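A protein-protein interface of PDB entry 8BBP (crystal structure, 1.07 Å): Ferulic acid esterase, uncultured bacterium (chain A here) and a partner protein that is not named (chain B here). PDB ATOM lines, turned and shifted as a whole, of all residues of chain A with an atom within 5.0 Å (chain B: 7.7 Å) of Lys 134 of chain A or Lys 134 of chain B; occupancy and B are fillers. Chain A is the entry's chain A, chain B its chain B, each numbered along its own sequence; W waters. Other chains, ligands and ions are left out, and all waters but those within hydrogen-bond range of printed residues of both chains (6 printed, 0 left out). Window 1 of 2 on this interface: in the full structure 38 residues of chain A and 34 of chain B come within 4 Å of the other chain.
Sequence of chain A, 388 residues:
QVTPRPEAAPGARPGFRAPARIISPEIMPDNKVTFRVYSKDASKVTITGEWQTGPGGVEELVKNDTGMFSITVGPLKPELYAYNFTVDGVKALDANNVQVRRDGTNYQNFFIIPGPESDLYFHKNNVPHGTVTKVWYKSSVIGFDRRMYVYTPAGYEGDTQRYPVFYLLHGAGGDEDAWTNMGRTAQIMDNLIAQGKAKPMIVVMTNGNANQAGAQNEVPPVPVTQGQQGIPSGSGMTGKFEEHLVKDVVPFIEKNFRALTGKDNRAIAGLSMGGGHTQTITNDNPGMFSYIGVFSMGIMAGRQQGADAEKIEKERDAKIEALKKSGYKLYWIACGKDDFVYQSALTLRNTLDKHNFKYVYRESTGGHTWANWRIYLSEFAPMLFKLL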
ATOM      1  N   GLY A 130      34.395  -8.778 -24.305  1.00  0.00           N
ATOM      2  CA  GLY A 130      34.607  -7.793 -25.336  1.00  0.00           C
ATOM      3  C   GLY A 130      33.560  -6.697 -25.322  1.00  0.00           C
ATOM      4  O   GLY A 130      32.427  -6.877 -24.894  1.00  0.00           O
ATOM      5  N   THR A 131      33.961  -5.546 -25.833  1.00  0.00           N
ATOM      6  CA  THR A 131      33.087  -4.392 -25.952  1.00  0.00           C
ATOM      7  C   THR A 131      32.107  -4.566 -27.099  1.00  0.00           C
ATOM      8  O   THR A 131      32.453  -5.122 -28.141  1.00  0.00           O
ATOM      9  CB  THR A 131      33.962  -3.165 -26.188  1.00  0.00           C
ATOM     10  OG1 THR A 131      34.765  -3.016 -25.023  1.00  0.00           O
ATOM     11  CG2 THR A 131      33.167  -1.891 -26.427  1.00  0.00           C
ATOM     12  N   VAL A 132      30.888  -4.072 -26.903  1.00  0.00           N
ATOM     13  CA  VAL A 132      29.906  -3.935 -27.973  1.00  0.00           C
ATOM     14  C   VAL A 132      29.649  -2.449 -28.150  1.00  0.00           C
ATOM     15  O   VAL A 132      29.229  -1.763 -27.206  1.00  0.00           O
ATOM     16  CB  VAL A 132      28.604  -4.698 -27.688  1.00  0.00           C
ATOM     17  CG1 VAL A 132      27.617  -4.471 -28.817  1.00  0.00           C
ATOM     18  CG2 VAL A 132      28.897  -6.164 -27.509  1.00  0.00           C
ATOM     19  N   THR A 133      29.911  -1.957 -29.353  1.00  0.00           N
ATOM     20  CA  THR A 133      29.827  -0.553 -29.699  1.00  0.00           C
ATOM     21  C   THR A 133      28.709  -0.356 -30.714  1.00  0.00           C
ATOM     22  O   THR A 133      28.689  -1.011 -31.756  1.00  0.00           O
ATOM     23  CB  THR A 133      31.165  -0.099 -30.299  1.00  0.00           C
ATOM     24  OG1 THR A 133      32.204  -0.242 -29.327  1.00  0.00           O
ATOM     25  CG2 THR A 133      31.116   1.333 -30.738  1.00  0.00           C
ATOM     26  N   LYS A 134      27.785   0.547 -30.414  1.00  0.00           N
ATOM     27  CA  LYS A 134      26.681   0.894 -31.310  1.00  0.00           C
ATOM     28  C   LYS A 134      27.072   2.217 -31.956  1.00  0.00           C
ATOM     29  O   LYS A 134      26.979   3.274 -31.328  1.00  0.00           O
ATOM     30  CB  LYS A 134      25.377   1.018 -30.534  1.00  0.00           C
ATOM     31  CG  LYS A 134      25.040  -0.169 -29.665  1.00  0.00           C
ATOM     32  CD  LYS A 134      23.615  -0.041 -29.175  1.00  0.00           C
ATOM     33  CE  LYS A 134      23.220  -1.078 -28.168  1.00  0.00           C
ATOM     34  NZ  LYS A 134      21.724  -1.113 -27.995  1.00  0.00           N
ATOM     35  N   VAL A 135      27.569   2.144 -33.186  1.00  0.00           N
ATOM     36  CA  VAL A 135      28.240   3.260 -33.834  1.00  0.00           C
ATOM     37  C   VAL A 135      27.534   3.614 -35.130  1.00  0.00           C
ATOM     38  O   VAL A 135      27.113   2.732 -35.888  1.00  0.00           O
ATOM     39  CB  VAL A 135      29.740   2.950 -34.055  1.00  0.00           C
ATOM     40  CG1 VAL A 135      29.946   1.648 -34.820  1.00  0.00           C
ATOM     41  CG2 VAL A 135      30.452   4.106 -34.740  1.00  0.00           C
ATOM     42  N   TRP A 136      27.425   4.917 -35.386  1.00  0.00           N
ATOM     43  CA  TRP A 136      26.844   5.451 -36.600  1.00  0.00           C
ATOM     44  C   TRP A 136      27.928   5.837 -37.591  1.00  0.00           C
ATOM     45  O   TRP A 136      29.034   6.228 -37.216  1.00  0.00           O
ATOM     46  CB  TRP A 136      25.981   6.666 -36.277  1.00  0.00           C
ATOM     47  CG  TRP A 136      24.779   6.306 -35.473  1.00  0.00           C
ATOM     48  CD1 TRP A 136      24.721   6.071 -34.125  1.00  0.00           C
ATOM     49  CD2 TRP A 136      23.449   6.129 -35.971  1.00  0.00           C
ATOM     50  NE1 TRP A 136      23.425   5.770 -33.751  1.00  0.00           N
ATOM     51  CE2 TRP A 136      22.630   5.804 -34.870  1.00  0.00           C
ATOM     52  CE3 TRP A 136      22.867   6.223 -37.241  1.00  0.00           C
ATOM     53  CZ2 TRP A 136      21.266   5.551 -35.005  1.00  0.00           C
ATOM     54  CZ3 TRP A 136      21.510   5.993 -37.372  1.00  0.00           C
ATOM     55  CH2 TRP A 136      20.726   5.644 -36.258  1.00  0.00           C
ATOM     56  N   ARG A 147      23.400   2.846 -38.426  1.00  0.00           N
ATOM     57  CA  ARG A 147      23.967   2.302 -37.206  1.00  0.00           C
ATOM     58  C   ARG A 147      24.371   0.854 -37.415  1.00  0.00           C
ATOM     59  O   ARG A 147      23.649   0.081 -38.058  1.00  0.00           O
ATOM     60  CB  ARG A 147      22.968   2.390 -36.052  1.00  0.00           C
ATOM     61  CG  ARG A 147      23.605   2.230 -34.693  1.00  0.00           C
ATOM     62  CD  ARG A 147      22.639   2.368 -33.539  1.00  0.00           C
ATOM     63  NE  ARG A 147      21.712   1.249 -33.493  1.00  0.00           N
ATOM     64  CZ  ARG A 147      20.931   0.961 -32.467  1.00  0.00           C
ATOM     65  NH1 ARG A 147      21.001   1.642 -31.339  1.00  0.00           N
ATOM     66  NH2 ARG A 147      20.063  -0.037 -32.582  1.00  0.00           N
ATOM     67  N   MET A 148      25.510   0.480 -36.840  1.00  0.00           N
ATOM     68  CA  MET A 148      25.932  -0.909 -36.790  1.00  0.00           C
ATOM     69  C   MET A 148      26.421  -1.213 -35.385  1.00  0.00           C
ATOM     70  O   MET A 148      26.693  -0.309 -34.590  1.00  0.00           O
ATOM     71  CB  MET A 148      27.023  -1.223 -37.818  1.00  0.00           C
ATOM     72  CG  MET A 148      28.267  -0.349 -37.706  1.00  0.00           C
ATOM     73  SD  MET A 148      29.390  -0.770 -39.039  1.00  0.00           S
ATOM     74  CE  MET A 148      30.507   0.625 -38.968  1.00  0.00           C
ATOM     75  N   TYR A 149      26.514  -2.495 -35.071  1.00  0.00           N
ATOM     76  CA  TYR A 149      27.113  -2.955 -33.830  1.00  0.00           C
ATOM     77  C   TYR A 149      28.474  -3.547 -34.143  1.00  0.00           C
ATOM     78  O   TYR A 149      28.605  -4.345 -35.072  1.00  0.00           O
ATOM     79  CB  TYR A 149      26.292  -4.038 -33.139  1.00  0.00           C
ATOM     80  CG  TYR A 149      25.057  -3.616 -32.383  1.00  0.00           C
ATOM     81  CD1 TYR A 149      24.318  -2.494 -32.725  1.00  0.00           C
ATOM     82  CD2 TYR A 149      24.609  -4.390 -31.336  1.00  0.00           C
ATOM     83  CE1 TYR A 149      23.154  -2.166 -32.038  1.00  0.00           C
ATOM     84  CE2 TYR A 149      23.449  -4.073 -30.655  1.00  0.00           C
ATOM     85  CZ  TYR A 149      22.724  -2.974 -31.027  1.00  0.00           C
ATOM     86  OH  TYR A 149      21.552  -2.656 -30.375  1.00  0.00           O
ATOM     87  N   ASP A 177      21.037  -5.209 -34.283  1.00  0.00           N
ATOM     88  CA  ASP A 177      20.994  -5.738 -32.925  1.00  0.00           C
ATOM     89  C   ASP A 177      20.795  -7.250 -32.884  1.00  0.00           C
ATOM     90  O   ASP A 177      21.023  -7.864 -31.845  1.00  0.00           O
ATOM     91  CB  ASP A 177      19.831  -5.012 -32.218  1.00  0.00           C
ATOM     92  CG  ASP A 177      19.597  -5.437 -30.773  1.00  0.00           C
ATOM     93  OD1 ASP A 177      20.372  -5.014 -29.894  1.00  0.00           O
ATOM     94  OD2 ASP A 177      18.581  -6.119 -30.517  1.00  0.00           O
ATOM     95  N   GLU A 218      14.438   1.301 -31.852  1.00  0.00           N
ATOM     96  CA  GLU A 218      15.118   2.511 -31.404  1.00  0.00           C
ATOM     97  C   GLU A 218      15.124   3.626 -32.424  1.00  0.00           C
ATOM     98  O   GLU A 218      15.260   4.789 -32.035  1.00  0.00           O
ATOM     99  CB  GLU A 218      16.583   2.206 -31.091  1.00  0.00           C
ATOM    100  CG  GLU A 218      16.777   1.191 -30.014  1.00  0.00           C
ATOM    101  CD  GLU A 218      18.224   1.068 -29.628  1.00  0.00           C
ATOM    102  OE1 GLU A 218      18.765   2.070 -29.118  1.00  0.00           O
ATOM    103  OE2 GLU A 218      18.828   0.000 -29.867  1.00  0.00           O
ATOM    104  N   HIS B 129      24.362  11.166 -34.738  1.00  0.00           N
ATOM    105  CA  HIS B 129      24.192  10.357 -33.538  1.00  0.00           C
ATOM    106  C   HIS B 129      25.514   9.911 -32.940  1.00  0.00           C
ATOM    107  O   HIS B 129      26.382   9.380 -33.640  1.00  0.00           O
ATOM    108  CB  HIS B 129      23.312   9.142 -33.823  1.00  0.00           C
ATOM    109  CG  HIS B 129      21.958   9.517 -34.298  1.00  0.00           C
ATOM    110  ND1 HIS B 129      21.131  10.346 -33.577  1.00  0.00           N
ATOM    111  CD2 HIS B 129      21.307   9.244 -35.450  1.00  0.00           C
ATOM    112  CE1 HIS B 129      20.016  10.550 -34.249  1.00  0.00           C
ATOM    113  NE2 HIS B 129      20.095   9.888 -35.390  1.00  0.00           N
ATOM    114  N   GLY B 130      25.629  10.093 -31.631  1.00  0.00           N
ATOM    115  CA  GLY B 130      26.776   9.631 -30.910  1.00  0.00           C
ATOM    116  C   GLY B 130      26.755   8.136 -30.658  1.00  0.00           C
ATOM    117  O   GLY B 130      25.708   7.505 -30.551  1.00  0.00           O
ATOM    118  N   THR B 131      27.950   7.580 -30.523  1.00  0.00           N
ATOM    119  CA  THR B 131      28.134   6.170 -30.239  1.00  0.00           C
ATOM    120  C   THR B 131      27.818   5.877 -28.785  1.00  0.00           C
ATOM    121  O   THR B 131      28.106   6.678 -27.893  1.00  0.00           O
ATOM    122  CB  THR B 131      29.583   5.810 -30.546  1.00  0.00           C
ATOM    123  OG1 THR B 131      29.777   6.003 -31.941  1.00  0.00           O
ATOM    124  CG2 THR B 131      29.926   4.389 -30.193  1.00  0.00           C
ATOM    125  N   VAL B 132      27.244   4.707 -28.550  1.00  0.00           N
ATOM    126  CA  VAL B 132      27.097   4.144 -27.218  1.00  0.00           C
ATOM    127  C   VAL B 132      27.920   2.872 -27.171  1.00  0.00           C
ATOM    128  O   VAL B 132      27.692   1.946 -27.958  1.00  0.00           O
ATOM    129  CB  VAL B 132      25.634   3.875 -26.841  1.00  0.00           C
ATOM    130  CG1 VAL B 132      25.560   3.256 -25.476  1.00  0.00           C
ATOM    131  CG2 VAL B 132      24.824   5.165 -26.889  1.00  0.00           C
ATOM    132  N   THR B 133      28.889   2.846 -26.270  1.00  0.00           N
ATOM    133  CA  THR B 133      29.842   1.764 -26.126  1.00  0.00           C
ATOM    134  C   THR B 133      29.604   1.067 -24.792  1.00  0.00           C
ATOM    135  O   THR B 133      29.609   1.708 -23.737  1.00  0.00           O
ATOM    136  CB  THR B 133      31.258   2.349 -26.173  1.00  0.00           C
ATOM    137  OG1 THR B 133      31.454   3.009 -27.427  1.00  0.00           O
ATOM    138  CG2 THR B 133      32.296   1.271 -26.025  1.00  0.00           C
ATOM    139  N   LYS B 134      29.409  -0.243 -24.833  1.00  0.00           N
ATOM    140  CA  LYS B 134      29.240  -1.060 -23.637  1.00  0.00           C
ATOM    141  C   LYS B 134      30.577  -1.745 -23.401  1.00  0.00           C
ATOM    142  O   LYS B 134      30.919  -2.716 -24.077  1.00  0.00           O
ATOM    143  CB  LYS B 134      28.121  -2.075 -23.822  1.00  0.00           C
ATOM    144  CG  LYS B 134      26.816  -1.508 -24.323  1.00  0.00           C
ATOM    145  CD  LYS B 134      25.722  -2.561 -24.210  1.00  0.00           C
ATOM    146  CE  LYS B 134      24.418  -2.182 -24.843  1.00  0.00           C
ATOM    147  NZ  LYS B 134      23.326  -3.099 -24.383  1.00  0.00           N
ATOM    148  N   VAL B 135      31.354  -1.209 -22.471  1.00  0.00           N
ATOM    149  CA  VAL B 135      32.761  -1.553 -22.318  1.00  0.00           C
ATOM    150  C   VAL B 135      33.022  -2.089 -20.923  1.00  0.00           C
ATOM    151  O   VAL B 135      32.476  -1.581 -19.937  1.00  0.00           O
ATOM    152  CB  VAL B 135      33.671  -0.347 -22.655  1.00  0.00           C
ATOM    153  CG1 VAL B 135      33.316   0.900 -21.836  1.00  0.00           C
ATOM    154  CG2 VAL B 135      35.146  -0.702 -22.486  1.00  0.00           C
ATOM    155  N   TRP B 136      33.868  -3.107 -20.848  1.00  0.00           N
ATOM    156  CA  TRP B 136      34.280  -3.713 -19.595  1.00  0.00           C
ATOM    157  C   TRP B 136      35.642  -3.183 -19.181  1.00  0.00           C
ATOM    158  O   TRP B 136      36.484  -2.845 -20.014  1.00  0.00           O
ATOM    159  CB  TRP B 136      34.329  -5.237 -19.721  1.00  0.00           C
ATOM    160  CG  TRP B 136      32.981  -5.833 -19.916  1.00  0.00           C
ATOM    161  CD1 TRP B 136      32.261  -5.895 -21.080  1.00  0.00           C
ATOM    162  CD2 TRP B 136      32.179  -6.459 -18.918  1.00  0.00           C
ATOM    163  NE1 TRP B 136      31.059  -6.517 -20.854  1.00  0.00           N
ATOM    164  CE2 TRP B 136      30.988  -6.881 -19.537  1.00  0.00           C
ATOM    165  CE3 TRP B 136      32.355  -6.702 -17.553  1.00  0.00           C
ATOM    166  CZ2 TRP B 136      29.972  -7.510 -18.836  1.00  0.00           C
ATOM    167  CZ3 TRP B 136      31.350  -7.345 -16.859  1.00  0.00           C
ATOM    168  CH2 TRP B 136      30.172  -7.740 -17.505  1.00  0.00           C
ATOM    169  N   ARG B 146      33.968  -5.024 -14.580  1.00  0.00           N
ATOM    170  CA  ARG B 146      32.631  -4.454 -14.569  1.00  0.00           C
ATOM    171  C   ARG B 146      32.352  -3.782 -15.904  1.00  0.00           C
ATOM    172  O   ARG B 146      33.271  -3.462 -16.661  1.00  0.00           O
ATOM    173  CB  ARG B 146      32.484  -3.439 -13.427  1.00  0.00           C
ATOM    174  CG  ARG B 146      32.931  -4.015 -12.107  1.00  0.00           C
ATOM    175  CD  ARG B 146      32.663  -3.095 -10.922  1.00  0.00           C
ATOM    176  NE  ARG B 146      31.245  -3.074 -10.573  1.00  0.00           N
ATOM    177  CZ  ARG B 146      30.436  -2.026 -10.678  1.00  0.00           C
ATOM    178  NH1 ARG B 146      30.852  -0.862 -11.143  1.00  0.00           N
ATOM    179  NH2 ARG B 146      29.171  -2.152 -10.303  1.00  0.00           N
ATOM    180  N   ARG B 147      31.068  -3.582 -16.191  1.00  0.00           N
ATOM    181  CA  ARG B 147      30.622  -2.983 -17.434  1.00  0.00           C
ATOM    182  C   ARG B 147      30.073  -1.587 -17.187  1.00  0.00           C
ATOM    183  O   ARG B 147      29.353  -1.355 -16.216  1.00  0.00           O
ATOM    184  CB  ARG B 147      29.534  -3.841 -18.097  1.00  0.00           C
ATOM    185  CG  ARG B 147      29.364  -3.538 -19.566  1.00  0.00           C
ATOM    186  CD  ARG B 147      28.328  -4.411 -20.266  1.00  0.00           C
ATOM    187  NE  ARG B 147      26.989  -4.134 -19.767  1.00  0.00           N
ATOM    188  CZ  ARG B 147      25.870  -4.546 -20.343  1.00  0.00           C
ATOM    189  NH1 ARG B 147      25.882  -5.198 -21.490  1.00  0.00           N
ATOM    190  NH2 ARG B 147      24.708  -4.295 -19.750  1.00  0.00           N
ATOM    191  N   MET B 148      30.376  -0.670 -18.103  1.00  0.00           N
ATOM    192  CA  MET B 148      29.779   0.655 -18.117  1.00  0.00           C
ATOM    193  C   MET B 148      29.363   0.992 -19.540  1.00  0.00           C
ATOM    194  O   MET B 148      29.790   0.345 -20.501  1.00  0.00           O
ATOM    195  CB  MET B 148      30.729   1.723 -17.546  1.00  0.00           C
ATOM    196  CG  MET B 148      32.049   1.811 -18.270  1.00  0.00           C
ATOM    197  SD  MET B 148      33.059   3.068 -17.464  1.00  0.00           S
ATOM    198  CE  MET B 148      34.652   2.678 -18.183  1.00  0.00           C
ATOM    199  N   TYR B 149      28.504   1.996 -19.671  1.00  0.00           N
ATOM    200  CA  TYR B 149      28.141   2.540 -20.970  1.00  0.00           C
ATOM    201  C   TYR B 149      28.803   3.894 -21.135  1.00  0.00           C
ATOM    202  O   TYR B 149      28.757   4.728 -20.230  1.00  0.00           O
ATOM    203  CB  TYR B 149      26.638   2.752 -21.126  1.00  0.00           C
ATOM    204  CG  TYR B 149      25.767   1.543 -21.376  1.00  0.00           C
ATOM    205  CD1 TYR B 149      26.113   0.278 -20.946  1.00  0.00           C
ATOM    206  CD2 TYR B 149      24.550   1.707 -21.995  1.00  0.00           C
ATOM    207  CE1 TYR B 149      25.251  -0.798 -21.134  1.00  0.00           C
ATOM    208  CE2 TYR B 149      23.692   0.645 -22.203  1.00  0.00           C
ATOM    209  CZ  TYR B 149      24.043  -0.598 -21.745  1.00  0.00           C
ATOM    210  OH  TYR B 149      23.192  -1.673 -21.915  1.00  0.00           O
ATOM    211  N   VAL B 150      29.384   4.126 -22.303  1.00  0.00           N
ATOM    212  CA  VAL B 150      30.016   5.400 -22.596  1.00  0.00           C
ATOM    213  C   VAL B 150      29.411   5.955 -23.871  1.00  0.00           C
ATOM    214  O   VAL B 150      29.423   5.293 -24.918  1.00  0.00           O
ATOM    215  CB  VAL B 150      31.535   5.263 -22.749  1.00  0.00           C
ATOM    216  CG1 VAL B 150      32.151   6.620 -23.018  1.00  0.00           C
ATOM    217  CG2 VAL B 150      32.147   4.624 -21.517  1.00  0.00           C
ATOM    218  N   TYR B 151      28.881   7.163 -23.784  1.00  0.00           N
ATOM    219  CA  TYR B 151      28.407   7.917 -24.927  1.00  0.00           C
ATOM    220  C   TYR B 151      29.527   8.833 -25.388  1.00  0.00           C
ATOM    221  O   TYR B 151      30.115   9.559 -24.580  1.00  0.00           O
ATOM    222  CB  TYR B 151      27.206   8.763 -24.516  1.00  0.00           C
ATOM    223  CG  TYR B 151      26.747   9.757 -25.557  1.00  0.00           C
ATOM    224  CD1 TYR B 151      27.273  11.039 -25.608  1.00  0.00           C
ATOM    225  CD2 TYR B 151      25.751   9.438 -26.466  1.00  0.00           C
ATOM    226  CE1 TYR B 151      26.846  11.953 -26.535  1.00  0.00           C
ATOM    227  CE2 TYR B 151      25.311  10.356 -27.395  1.00  0.00           C
ATOM    228  CZ  TYR B 151      25.871  11.614 -27.433  1.00  0.00           C
ATOM    229  OH  TYR B 151      25.438  12.553 -28.338  1.00  0.00           O
ATOM    230  N   THR B 152      29.819   8.790 -26.682  1.00  0.00           N
ATOM    231  CA  THR B 152      30.716   9.757 -27.281  1.00  0.00           C
ATOM    232  C   THR B 152      29.924  10.593 -28.276  1.00  0.00           C
ATOM    233  O   THR B 152      28.955  10.114 -28.874  1.00  0.00           O
ATOM    234  CB  THR B 152      31.927   9.105 -27.961  1.00  0.00           C
ATOM    235  OG1 THR B 152      31.490   8.036 -28.804  1.00  0.00           O
ATOM    236  CG2 THR B 152      32.888   8.531 -26.946  1.00  0.00           C
ATOM    237  N   GLU B 157      34.328   9.566 -33.939  1.00  0.00           N
ATOM    238  CA  GLU B 157      35.073   8.683 -34.820  1.00  0.00           C
ATOM    239  C   GLU B 157      35.545   9.451 -36.040  1.00  0.00           C
ATOM    240  O   GLU B 157      34.756  10.119 -36.714  1.00  0.00           O
ATOM    241  CB  GLU B 157      34.189   7.512 -35.247  1.00  0.00           C
ATOM    242  CG  GLU B 157      33.866   6.524 -34.123  1.00  0.00           C
ATOM    243  CD  GLU B 157      32.682   6.916 -33.244  1.00  0.00           C
ATOM    244  OE1 GLU B 157      32.059   7.999 -33.420  1.00  0.00           O
ATOM    245  OE2 GLU B 157      32.372   6.116 -32.350  1.00  0.00           O
ATOM    246  N   GLU B 176      24.038   0.269 -15.354  1.00  0.00           N
ATOM    247  CA  GLU B 176      24.708   1.085 -16.355  1.00  0.00           C
ATOM    248  C   GLU B 176      23.870   1.317 -17.603  1.00  0.00           C
ATOM    249  O   GLU B 176      24.227   2.187 -18.404  1.00  0.00           O
ATOM    250  CB  GLU B 176      26.062   0.466 -16.729  1.00  0.00           C
ATOM    251  CG  GLU B 176      26.009  -0.859 -17.525  1.00  0.00           C
ATOM    252  CD  GLU B 176      25.745  -2.116 -16.717  1.00  0.00           C
ATOM    253  OE1 GLU B 176      25.874  -3.212 -17.323  1.00  0.00           O
ATOM    254  OE2 GLU B 176      25.407  -2.047 -15.510  1.00  0.00           O
ATOM    255  N   ASP B 177      22.800   0.543 -17.811  1.00  0.00           N
ATOM    256  CA  ASP B 177      21.901   0.713 -18.944  1.00  0.00           C
ATOM    257  C   ASP B 177      20.805   1.746 -18.688  1.00  0.00           C
ATOM    258  O   ASP B 177      20.169   2.214 -19.633  1.00  0.00           O
ATOM    259  CB  ASP B 177      21.298  -0.674 -19.225  1.00  0.00           C
ATOM    260  CG  ASP B 177      20.310  -0.715 -20.390  1.00  0.00           C
ATOM    261  OD1 ASP B 177      20.749  -0.695 -21.557  1.00  0.00           O
ATOM    262  OD2 ASP B 177      19.095  -0.848 -20.112  1.00  0.00           O
ATOM    263  N   THR B 180      20.539   5.510 -20.361  1.00  0.00           N
ATOM    264  CA  THR B 180      20.143   5.511 -21.768  1.00  0.00           C
ATOM    265  C   THR B 180      18.746   4.953 -21.959  1.00  0.00           C
ATOM    266  O   THR B 180      17.970   5.502 -22.732  1.00  0.00           O
ATOM    267  CB  THR B 180      21.143   4.807 -22.681  1.00  0.00           C
ATOM    268  OG1 THR B 180      21.501   3.542 -22.145  1.00  0.00           O
ATOM    269  CG2 THR B 180      22.376   5.677 -22.913  1.00  0.00           C
ATOM    270  N   ASN B 217      19.864  -7.900 -16.440  1.00  0.00           N
ATOM    271  CA  ASN B 217      19.201  -8.563 -17.559  1.00  0.00           C
ATOM    272  C   ASN B 217      20.186  -9.248 -18.488  1.00  0.00           C
ATOM    273  O   ASN B 217      19.755 -10.032 -19.334  1.00  0.00           O
ATOM    274  CB  ASN B 217      18.340  -7.575 -18.347  1.00  0.00           C
ATOM    275  CG  ASN B 217      19.164  -6.511 -19.032  1.00  0.00           C
ATOM    276  OD1 ASN B 217      20.080  -5.946 -18.441  1.00  0.00           O
ATOM    277  ND2 ASN B 217      18.843  -6.232 -20.287  1.00  0.00           N
ATOM    278  N   GLU B 218      21.479  -8.961 -18.358  1.00  0.00           N
ATOM    279  CA  GLU B 218      22.509  -9.510 -19.226  1.00  0.00           C
ATOM    280  C   GLU B 218      23.620 -10.230 -18.484  1.00  0.00           C
ATOM    281  O   GLU B 218      24.284 -11.089 -19.065  1.00  0.00           O
ATOM    282  CB  GLU B 218      23.149  -8.396 -20.054  1.00  0.00           C
ATOM    283  CG  GLU B 218      22.198  -7.689 -20.980  1.00  0.00           C
ATOM    284  CD  GLU B 218      22.935  -6.703 -21.829  1.00  0.00           C
ATOM    285  OE1 GLU B 218      22.781  -5.478 -21.649  1.00  0.00           O
ATOM    286  OE2 GLU B 218      23.745  -7.162 -22.638  1.00  0.00           O
ATOM    287  N   PHE B 257      39.710   6.799 -24.047  1.00  0.00           N
ATOM    288  CA  PHE B 257      38.910   7.731 -24.821  1.00  0.00           C
ATOM    289  C   PHE B 257      39.687   9.029 -24.934  1.00  0.00           C
ATOM    290  O   PHE B 257      40.567   9.319 -24.122  1.00  0.00           O
ATOM    291  CB  PHE B 257      37.525   7.965 -24.184  1.00  0.00           C
ATOM    292  CG  PHE B 257      36.667   6.746 -24.187  1.00  0.00           C
ATOM    293  CD1 PHE B 257      36.817   5.782 -23.212  1.00  0.00           C
ATOM    294  CD2 PHE B 257      35.731   6.552 -25.181  1.00  0.00           C
ATOM    295  CE1 PHE B 257      36.058   4.641 -23.224  1.00  0.00           C
ATOM    296  CE2 PHE B 257      34.964   5.406 -25.196  1.00  0.00           C
ATOM    297  CZ  PHE B 257      35.122   4.460 -24.215  1.00  0.00           C
HETATM  298  O   HOH W   1      30.348  -5.434 -23.726  1.00  0.00           O
HETATM  299  O   HOH W   2      24.761   4.939 -31.017  1.00  0.00           O
HETATM  300  O   HOH W   3      30.408   7.978 -35.766  1.00  0.00           O
HETATM  301  O   HOH W   4      20.966  -2.640 -25.793  1.00  0.00           O
HETATM  302  O   HOH W   5      35.194  -4.657 -22.940  1.00  0.00           O
HETATM  303  O   HOH W   6      28.177   7.225 -33.755  1.00  0.00           O
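Water W5 lies within hydrogen-bond range of OG1 of Thr 131 of chain A and N of Trp 136 of chain B. Water W2 lies within hydrogen-bond range of O of Gly 130 of chain B (2.8 Å), O of Lys 134 of chain A (2.8 Å) and NE1 of Trp 136 of chain A (3.2 Å).
O of Val 135 of chain A sits at hydrogen-bond distance from N of Met 148 of chain A (2.9 Å). OE1 of Glu 218 of chain B lies within salt-bridge range of NZ of Lys 134 of chain B, at 3.7 Å.
Lys 134 of chain A touches three residues of chain B. Of chain A, only Thr 131, Val 132 and Lys 134 come within 4 Å of Lys 134 of chain B. Of the printed residues of chain B, Val 135 of chain A touches Thr 131 and Glu 157. Of the printed residues of chain B, Thr 133 of chain A touches Thr 131, Val 132 and Thr 133. Of the printed residues of chain A, Gly 130 of chain B touches Trp 136. The nearest residue of chain B that does not touch Lys 134 of chain A is Gly 130 of chain B (4.5 Å). The nearest residue of chain A that does not touch Lys 134 of chain B is Gly 130 of chain A (4.5 Å).
Among the printed residues, merely in contact across the chains: Gly 130 of chain A with Trp 136 of chain B (3.9 Å), Thr 131 of chain A with Thr 133 of chain B (3.3 Å), Thr 131 of chain A with Lys 134 of chain B (3.3 Å), Thr 131 of chain A with Val 135 of chain B (3.5 Å), Val 132 of chain A with Thr 133 of chain B (3.7 Å), Thr 133 of chain A with Thr 131 of chain B (3.3 Å), Thr 133 of chain A with Val 132 of chain B (3.7 Å), Thr 133 of chain A with Thr 133 of chain B (3.6 Å), Lys 134 of chain A with Thr 131 of chain B (3.3 Å), Lys 134 of chain A with Lys 134 of chain B (3.7 Å), Val 135 of chain A with Thr 131 of chain B (3.4 Å), Val 135 of chain A with Glu 157 of chain B (3.7 Å), Trp 136 of chain A with His 129 of chain B (3.4 Å) and Trp 136 of chain A with Gly 130 of chain B (3.98 Å).
Of the 22 printed residues of chain B, 9 touch a printed residue of chain A. Hydrophobic or aromatic side chains of chain B within 4 Å of the printed part of chain A: His 129, Val 135 and Trp 136. Of the 12 printed residues of chain A, 7 touch a printed residue of chain B. Among the printed residues, 16 pairs touch across the chains. Among the printed residues, no Asp or Glu carboxylate lies within 4 Å of a Lys or Arg side-chain nitrogen of the other chain.
The backbone NH (N) of Lys 134 of chain B is in hydrogen-bond range of the backbone carbonyl oxygen (O) of Val 132 of chain A, at 2.8 Å. The backbone NH of Lys 134 of chain A lies within hydrogen-bond range of the backbone carbonyl oxygen of Val 132 of chain B, 2.8 Å away.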
